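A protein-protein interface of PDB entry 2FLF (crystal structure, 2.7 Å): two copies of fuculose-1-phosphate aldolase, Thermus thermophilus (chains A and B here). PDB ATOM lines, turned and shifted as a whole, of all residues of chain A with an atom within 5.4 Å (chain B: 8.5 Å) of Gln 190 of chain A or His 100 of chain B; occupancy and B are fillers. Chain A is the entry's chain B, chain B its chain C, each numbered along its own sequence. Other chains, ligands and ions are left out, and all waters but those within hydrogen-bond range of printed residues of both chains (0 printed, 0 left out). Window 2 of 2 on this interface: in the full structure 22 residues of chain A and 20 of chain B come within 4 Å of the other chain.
Hydrophobic or aromatic side chains of chain A that line the printed part of chain B: Tyr 185, His 186, Leu 188, Trp 189 and Ala 192. Along chain A the printed residues that touch a printed residue of chain B span positions 185 to 193. Of the 17 printed residues of chain B, 7 touch a printed residue of chain A. Printed residues of chain B that touch a printed residue of chain A: Ala 96, Leu 97, Phe 99, His 100, Leu 184, Arg 187 and Leu 188. Hydrophobic or aromatic side chains of chain B within 4 Å of the printed part of chain A: Ala 96, Leu 97, Phe 99, His 100, Leu 184 and Leu 188. Among the printed residues, 13 pairs touch across the chains.
Printed residues of chain B within 4 Å of Gln 190 of chain A: His 100 and Arg 187. His 100 of chain B touches two residues of chain A. No residue of chain B comes within 4 Å of Gly 191 of chain A. Of the printed residues of chain B, Tyr 185 of chain A touches Ala 96 and Leu 184. Printed residues of chain B within 4 Å of Leu 188 of chain A: Leu 188. Of the printed residues of chain A, Arg 187 of chain B touches Trp 189, Gln 190 and Gly 193. Of the printed residues of chain B, Ala 192 of chain A touches Leu 188 (3.7 Å). Printed residues of chain A within 4 Å of Leu 188 of chain B: Leu 188 and Ala 192. The nearest printed residue of chain B that does not touch Gln 190 of chain A is Leu 97 of chain B (6.2 Å). The nearest printed residue of chain A that does not touch His 100 of chain B is Trp 189 of chain A (5.9 Å).
O of Phe 99 of chain B is in hydrogen-bond range of NE of Arg 149 of chain B, at 3.3 Å.
Leu 188 of chain A touches its own counterpart, Leu 188 of chain B. Positions printed for both chains: 187 and 188.
Tyr 185 of chain A touches Leu 184 of chain B (CD2 to CD2, 3.96 Å). N of His 186 of chain A touches CB of Ala 96 of chain B (3.3 Å). CD1 of Phe 99 of chain B touches CD2 of His 186 of chain A, 3.6 Å away. His 186 of chain A touches His 100 of chain B. Leu 188 of chain B touches Leu 188 of chain A. Trp 189 of chain A touches Leu 97 of chain B (CD2 to CD2, 3.2 Å). CE3 of Trp 189 of chain A touches CD1 of Leu 184 of chain B (3.8 Å). Gln 190 of chain A touches Arg 187 of chain B. CB of Ala 192 of chain A touches CD2 of Leu 188 of chain B, at 3.7 Å. Gly 193 of chain A touches Arg 187 of chain B.
O of Trp 189 of chain A lies close to NH2 of Arg 187 of chain B, 3.1 Å away. A ring nitrogen (ND1) of His 100 of chain B sits close to the side-chain amide oxygen (OE1) of Gln 190 of chain A (3.4 Å).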
ATOM      1  N   TYR A 185      33.658  -0.926  23.133  1.00  0.00           N
ATOM      2  CA  TYR A 185      32.450  -1.648  23.540  1.00  0.00           C
ATOM      3  C   TYR A 185      31.256  -0.699  23.664  1.00  0.00           C
ATOM      4  O   TYR A 185      30.182  -0.980  23.149  1.00  0.00           O
ATOM      5  CB  TYR A 185      32.671  -2.376  24.876  1.00  0.00           C
ATOM      6  CG  TYR A 185      33.871  -3.305  24.886  1.00  0.00           C
ATOM      7  CD1 TYR A 185      34.777  -3.285  25.936  1.00  0.00           C
ATOM      8  CD2 TYR A 185      34.117  -4.170  23.827  1.00  0.00           C
ATOM      9  CE1 TYR A 185      35.894  -4.090  25.930  1.00  0.00           C
ATOM     10  CE2 TYR A 185      35.228  -4.985  23.813  1.00  0.00           C
ATOM     11  CZ  TYR A 185      36.111  -4.936  24.872  1.00  0.00           C
ATOM     12  OH  TYR A 185      37.214  -5.746  24.879  1.00  0.00           O
ATOM     13  N   HIS A 186      31.429   0.426  24.341  1.00  0.00           N
ATOM     14  CA  HIS A 186      30.325   1.362  24.451  1.00  0.00           C
ATOM     15  C   HIS A 186      29.727   1.602  23.063  1.00  0.00           C
ATOM     16  O   HIS A 186      28.531   1.407  22.840  1.00  0.00           O
ATOM     17  CB  HIS A 186      30.809   2.681  25.031  1.00  0.00           C
ATOM     18  CG  HIS A 186      29.735   3.716  25.160  1.00  0.00           C
ATOM     19  ND1 HIS A 186      29.510   4.679  24.203  1.00  0.00           N
ATOM     20  CD2 HIS A 186      28.823   3.937  26.136  1.00  0.00           C
ATOM     21  CE1 HIS A 186      28.508   5.449  24.585  1.00  0.00           C
ATOM     22  NE2 HIS A 186      28.072   5.022  25.755  1.00  0.00           N
ATOM     23  N   ARG A 187      30.574   1.996  22.123  1.00  0.00           N
ATOM     24  CA  ARG A 187      30.122   2.274  20.783  1.00  0.00           C
ATOM     25  C   ARG A 187      29.517   1.097  20.010  1.00  0.00           C
ATOM     26  O   ARG A 187      28.445   1.220  19.426  1.00  0.00           O
ATOM     27  CB  ARG A 187      31.254   2.898  19.988  1.00  0.00           C
ATOM     28  CG  ARG A 187      30.806   3.340  18.622  1.00  0.00           C
ATOM     29  CD  ARG A 187      31.517   4.577  18.190  1.00  0.00           C
ATOM     30  NE  ARG A 187      31.448   4.672  16.748  1.00  0.00           N
ATOM     31  CZ  ARG A 187      32.017   5.636  16.048  1.00  0.00           C
ATOM     32  NH1 ARG A 187      32.691   6.586  16.671  1.00  0.00           N
ATOM     33  NH2 ARG A 187      31.913   5.644  14.730  1.00  0.00           N
ATOM     34  N   LEU A 188      30.181  -0.045  19.980  1.00  0.00           N
ATOM     35  CA  LEU A 188      29.606  -1.166  19.258  1.00  0.00           C
ATOM     36  C   LEU A 188      28.207  -1.488  19.793  1.00  0.00           C
ATOM     37  O   LEU A 188      27.356  -1.991  19.072  1.00  0.00           O
ATOM     38  CB  LEU A 188      30.489  -2.399  19.405  1.00  0.00           C
ATOM     39  CG  LEU A 188      31.844  -2.373  18.727  1.00  0.00           C
ATOM     40  CD1 LEU A 188      32.345  -3.791  18.605  1.00  0.00           C
ATOM     41  CD2 LEU A 188      31.727  -1.772  17.360  1.00  0.00           C
ATOM     42  N   TRP A 189      27.988  -1.180  21.064  1.00  0.00           N
ATOM     43  CA  TRP A 189      26.727  -1.442  21.753  1.00  0.00           C
ATOM     44  C   TRP A 189      25.639  -0.416  21.476  1.00  0.00           C
ATOM     45  O   TRP A 189      24.618  -0.728  20.862  1.00  0.00           O
ATOM     46  CB  TRP A 189      26.990  -1.518  23.260  1.00  0.00           C
ATOM     47  CG  TRP A 189      25.777  -1.604  24.128  1.00  0.00           C
ATOM     48  CD1 TRP A 189      25.112  -0.575  24.711  1.00  0.00           C
ATOM     49  CD2 TRP A 189      25.119  -2.799  24.555  1.00  0.00           C
ATOM     50  NE1 TRP A 189      24.086  -1.049  25.483  1.00  0.00           N
ATOM     51  CE2 TRP A 189      24.065  -2.413  25.404  1.00  0.00           C
ATOM     52  CE3 TRP A 189      25.321  -4.162  24.301  1.00  0.00           C
ATOM     53  CZ2 TRP A 189      23.216  -3.336  26.005  1.00  0.00           C
ATOM     54  CZ3 TRP A 189      24.483  -5.079  24.894  1.00  0.00           C
ATOM     55  CH2 TRP A 189      23.439  -4.662  25.737  1.00  0.00           C
ATOM     56  N   GLN A 190      25.850   0.802  21.959  1.00  0.00           N
ATOM     57  CA  GLN A 190      24.891   1.874  21.748  1.00  0.00           C
ATOM     58  C   GLN A 190      24.591   1.994  20.250  1.00  0.00           C
ATOM     59  O   GLN A 190      23.475   2.345  19.856  1.00  0.00           O
ATOM     60  CB  GLN A 190      25.466   3.187  22.301  1.00  0.00           C
ATOM     61  CG  GLN A 190      24.812   4.461  21.802  1.00  0.00           C
ATOM     62  CD  GLN A 190      25.470   5.712  22.374  1.00  0.00           C
ATOM     63  OE1 GLN A 190      25.321   6.020  23.559  1.00  0.00           O
ATOM     64  NE2 GLN A 190      26.212   6.434  21.532  1.00  0.00           N
ATOM     65  N   GLY A 191      25.579   1.648  19.426  1.00  0.00           N
ATOM     66  CA  GLY A 191      25.438   1.756  17.984  1.00  0.00           C
ATOM     67  C   GLY A 191      24.781   0.643  17.194  1.00  0.00           C
ATOM     68  O   GLY A 191      24.150   0.910  16.169  1.00  0.00           O
ATOM     69  N   ALA A 192      24.924  -0.600  17.641  1.00  0.00           N
ATOM     70  CA  ALA A 192      24.329  -1.717  16.920  1.00  0.00           C
ATOM     71  C   ALA A 192      22.989  -2.161  17.488  1.00  0.00           C
ATOM     72  O   ALA A 192      22.309  -2.982  16.880  1.00  0.00           O
ATOM     73  CB  ALA A 192      25.294  -2.892  16.889  1.00  0.00           C
ATOM     74  N   GLY A 193      22.605  -1.615  18.639  1.00  0.00           N
ATOM     75  CA  GLY A 193      21.344  -1.991  19.252  1.00  0.00           C
ATOM     76  C   GLY A 193      20.157  -1.242  18.660  1.00  0.00           C
ATOM     77  O   GLY A 193      20.190  -0.884  17.480  1.00  0.00           O
ATOM     78  N   ALA B  94      31.315  -4.462  30.912  1.00  0.00           N
ATOM     79  CA  ALA B  94      30.299  -4.111  31.886  1.00  0.00           C
ATOM     80  C   ALA B  94      30.144  -2.604  32.111  1.00  0.00           C
ATOM     81  O   ALA B  94      29.034  -2.121  32.259  1.00  0.00           O
ATOM     82  CB  ALA B  94      30.593  -4.798  33.184  1.00  0.00           C
ATOM     83  N   VAL B  95      31.251  -1.866  32.164  1.00  0.00           N
ATOM     84  CA  VAL B  95      31.169  -0.423  32.356  1.00  0.00           C
ATOM     85  C   VAL B  95      30.532   0.231  31.128  1.00  0.00           C
ATOM     86  O   VAL B  95      29.693   1.120  31.238  1.00  0.00           O
ATOM     87  CB  VAL B  95      32.559   0.190  32.597  1.00  0.00           C
ATOM     88  CG1 VAL B  95      32.577   1.632  32.174  1.00  0.00           C
ATOM     89  CG2 VAL B  95      32.909   0.098  34.052  1.00  0.00           C
ATOM     90  N   ALA B  96      30.929  -0.236  29.959  1.00  0.00           N
ATOM     91  CA  ALA B  96      30.401   0.284  28.718  1.00  0.00           C
ATOM     92  C   ALA B  96      28.883   0.116  28.629  1.00  0.00           C
ATOM     93  O   ALA B  96      28.189   1.029  28.199  1.00  0.00           O
ATOM     94  CB  ALA B  96      31.082  -0.399  27.542  1.00  0.00           C
ATOM     95  N   LEU B  97      28.363  -1.035  29.039  1.00  0.00           N
ATOM     96  CA  LEU B  97      26.926  -1.263  28.975  1.00  0.00           C
ATOM     97  C   LEU B  97      26.217  -0.602  30.137  1.00  0.00           C
ATOM     98  O   LEU B  97      25.001  -0.669  30.242  1.00  0.00           O
ATOM     99  CB  LEU B  97      26.601  -2.758  28.971  1.00  0.00           C
ATOM    100  CG  LEU B  97      27.335  -3.631  27.959  1.00  0.00           C
ATOM    101  CD1 LEU B  97      26.547  -4.878  27.710  1.00  0.00           C
ATOM    102  CD2 LEU B  97      27.534  -2.887  26.671  1.00  0.00           C
ATOM    103  N   SER B  98      26.973   0.050  31.004  1.00  0.00           N
ATOM    104  CA  SER B  98      26.383   0.706  32.162  1.00  0.00           C
ATOM    105  C   SER B  98      26.040   2.160  31.906  1.00  0.00           C
ATOM    106  O   SER B  98      25.198   2.731  32.587  1.00  0.00           O
ATOM    107  CB  SER B  98      27.343   0.641  33.340  1.00  0.00           C
ATOM    108  OG  SER B  98      27.651  -0.698  33.635  1.00  0.00           O
ATOM    109  N   PHE B  99      26.707   2.772  30.937  1.00  0.00           N
ATOM    110  CA  PHE B  99      26.452   4.173  30.647  1.00  0.00           C
ATOM    111  C   PHE B  99      25.004   4.516  30.336  1.00  0.00           C
ATOM    112  O   PHE B  99      24.606   5.660  30.495  1.00  0.00           O
ATOM    113  CB  PHE B  99      27.357   4.660  29.516  1.00  0.00           C
ATOM    114  CG  PHE B  99      28.749   4.943  29.963  1.00  0.00           C
ATOM    115  CD1 PHE B  99      29.804   4.115  29.586  1.00  0.00           C
ATOM    116  CD2 PHE B  99      29.007   6.022  30.818  1.00  0.00           C
ATOM    117  CE1 PHE B  99      31.098   4.361  30.056  1.00  0.00           C
ATOM    118  CE2 PHE B  99      30.289   6.278  31.290  1.00  0.00           C
ATOM    119  CZ  PHE B  99      31.337   5.445  30.912  1.00  0.00           C
ATOM    120  N   HIS B 100      24.211   3.538  29.908  1.00  0.00           N
ATOM    121  CA  HIS B 100      22.813   3.823  29.595  1.00  0.00           C
ATOM    122  C   HIS B 100      21.771   2.860  30.143  1.00  0.00           C
ATOM    123  O   HIS B 100      20.614   2.893  29.732  1.00  0.00           O
ATOM    124  CB  HIS B 100      22.639   3.997  28.083  1.00  0.00           C
ATOM    125  CG  HIS B 100      23.305   5.229  27.559  1.00  0.00           C
ATOM    126  ND1 HIS B 100      24.418   5.190  26.748  1.00  0.00           N
ATOM    127  CD2 HIS B 100      23.081   6.537  27.825  1.00  0.00           C
ATOM    128  CE1 HIS B 100      24.857   6.419  26.543  1.00  0.00           C
ATOM    129  NE2 HIS B 100      24.063   7.255  27.187  1.00  0.00           N
ATOM    130  N   LEU B 101      22.183   2.010  31.071  1.00  0.00           N
ATOM    131  CA  LEU B 101      21.266   1.076  31.705  1.00  0.00           C
ATOM    132  C   LEU B 101      21.036   1.609  33.112  1.00  0.00           C
ATOM    133  O   LEU B 101      21.675   2.563  33.548  1.00  0.00           O
ATOM    134  CB  LEU B 101      21.882  -0.316  31.842  1.00  0.00           C
ATOM    135  CG  LEU B 101      22.239  -1.228  30.676  1.00  0.00           C
ATOM    136  CD1 LEU B 101      22.731  -2.559  31.261  1.00  0.00           C
ATOM    137  CD2 LEU B 101      21.033  -1.439  29.770  1.00  0.00           C
ATOM    138  N   SER B 102      20.119   0.991  33.829  1.00  0.00           N
ATOM    139  CA  SER B 102      19.882   1.398  35.193  1.00  0.00           C
ATOM    140  C   SER B 102      20.229   0.141  35.981  1.00  0.00           C
ATOM    141  O   SER B 102      20.741   0.198  37.108  1.00  0.00           O
ATOM    142  CB  SER B 102      18.417   1.788  35.390  1.00  0.00           C
ATOM    143  OG  SER B 102      18.256   2.456  36.629  1.00  0.00           O
ATOM    144  N   ARG B 103      19.963  -0.989  35.331  1.00  0.00           N
ATOM    145  CA  ARG B 103      20.209  -2.318  35.858  1.00  0.00           C
ATOM    146  C   ARG B 103      20.814  -3.194  34.766  1.00  0.00           C
ATOM    147  O   ARG B 103      20.559  -2.998  33.572  1.00  0.00           O
ATOM    148  CB  ARG B 103      18.892  -2.932  36.329  1.00  0.00           C
ATOM    149  CG  ARG B 103      18.261  -2.114  37.466  1.00  0.00           C
ATOM    150  CD  ARG B 103      16.975  -2.775  38.053  1.00  0.00           C
ATOM    151  NE  ARG B 103      16.344  -1.944  39.114  1.00  0.00           N
ATOM    152  CZ  ARG B 103      15.120  -2.189  39.600  1.00  0.00           C
ATOM    153  NH1 ARG B 103      14.440  -3.227  39.114  1.00  0.00           N
ATOM    154  NH2 ARG B 103      14.561  -1.406  40.543  1.00  0.00           N
ATOM    155  N   VAL B 120      22.779  -0.374  38.541  1.00  0.00           N
ATOM    156  CA  VAL B 120      23.741   0.593  38.064  1.00  0.00           C
ATOM    157  C   VAL B 120      23.481   1.899  38.781  1.00  0.00           C
ATOM    158  O   VAL B 120      22.433   2.500  38.589  1.00  0.00           O
ATOM    159  CB  VAL B 120      23.572   0.864  36.563  1.00  0.00           C
ATOM    160  CG1 VAL B 120      24.601   1.872  36.091  1.00  0.00           C
ATOM    161  CG2 VAL B 120      23.683  -0.427  35.783  1.00  0.00           C
ATOM    162  N   ALA B 122      24.072   5.776  39.189  1.00  0.00           N
ATOM    163  CA  ALA B 122      24.490   6.799  38.245  1.00  0.00           C
ATOM    164  C   ALA B 122      24.219   8.197  38.743  1.00  0.00           C
ATOM    165  O   ALA B 122      23.197   8.802  38.406  1.00  0.00           O
ATOM    166  CB  ALA B 122      23.788   6.581  36.918  1.00  0.00           C
ATOM    167  N   ARG B 149      28.426   3.673  37.509  1.00  0.00           N
ATOM    168  CA  ARG B 149      28.591   4.290  36.193  1.00  0.00           C
ATOM    169  C   ARG B 149      29.910   4.991  35.931  1.00  0.00           C
ATOM    170  O   ARG B 149      30.261   5.975  36.575  1.00  0.00           O
ATOM    171  CB  ARG B 149      27.446   5.262  35.896  1.00  0.00           C
ATOM    172  CG  ARG B 149      27.496   5.805  34.478  1.00  0.00           C
ATOM    173  CD  ARG B 149      26.198   6.465  34.099  1.00  0.00           C
ATOM    174  NE  ARG B 149      25.154   5.500  33.771  1.00  0.00           N
ATOM    175  CZ  ARG B 149      23.854   5.773  33.804  1.00  0.00           C
ATOM    176  NH1 ARG B 149      22.959   4.851  33.486  1.00  0.00           N
ATOM    177  NH2 ARG B 149      23.446   6.969  34.177  1.00  0.00           N
ATOM    178  N   GLY B 150      30.637   4.459  34.964  1.00  0.00           N
ATOM    179  CA  GLY B 150      31.910   5.039  34.589  1.00  0.00           C
ATOM    180  C   GLY B 150      33.036   4.842  35.576  1.00  0.00           C
ATOM    181  O   GLY B 150      34.073   5.495  35.463  1.00  0.00           O
ATOM    182  N   LEU B 184      26.595  -8.447  25.310  1.00  0.00           N
ATOM    183  CA  LEU B 184      27.164  -7.743  24.173  1.00  0.00           C
ATOM    184  C   LEU B 184      27.152  -8.559  22.877  1.00  0.00           C
ATOM    185  O   LEU B 184      26.539  -8.157  21.902  1.00  0.00           O
ATOM    186  CB  LEU B 184      28.600  -7.283  24.499  1.00  0.00           C
ATOM    187  CG  LEU B 184      29.358  -6.637  23.326  1.00  0.00           C
ATOM    188  CD1 LEU B 184      28.638  -5.360  22.918  1.00  0.00           C
ATOM    189  CD2 LEU B 184      30.795  -6.328  23.704  1.00  0.00           C
ATOM    190  N   ARG B 187      23.989  -9.033  21.423  1.00  0.00           N
ATOM    191  CA  ARG B 187      23.437  -7.860  20.756  1.00  0.00           C
ATOM    192  C   ARG B 187      24.135  -7.547  19.443  1.00  0.00           C
ATOM    193  O   ARG B 187      23.507  -7.074  18.503  1.00  0.00           O
ATOM    194  CB  ARG B 187      23.494  -6.648  21.687  1.00  0.00           C
ATOM    195  CG  ARG B 187      22.923  -5.387  21.088  1.00  0.00           C
ATOM    196  CD  ARG B 187      22.116  -4.628  22.117  1.00  0.00           C
ATOM    197  NE  ARG B 187      22.598  -3.265  22.266  1.00  0.00           N
ATOM    198  CZ  ARG B 187      22.016  -2.343  23.025  1.00  0.00           C
ATOM    199  NH1 ARG B 187      20.916  -2.639  23.711  1.00  0.00           N
ATOM    200  NH2 ARG B 187      22.540  -1.124  23.102  1.00  0.00           N
ATOM    201  N   LEU B 188      25.429  -7.815  19.369  1.00  0.00           N
ATOM    202  CA  LEU B 188      26.171  -7.557  18.154  1.00  0.00           C
ATOM    203  C   LEU B 188      25.864  -8.618  17.120  1.00  0.00           C
ATOM    204  O   LEU B 188      25.612  -8.310  15.956  1.00  0.00           O
ATOM    205  CB  LEU B 188      27.666  -7.517  18.448  1.00  0.00           C
ATOM    206  CG  LEU B 188      28.122  -6.305  19.266  1.00  0.00           C
ATOM    207  CD1 LEU B 188      29.594  -6.426  19.577  1.00  0.00           C
ATOM    208  CD2 LEU B 188      27.845  -5.016  18.485  1.00  0.00           C
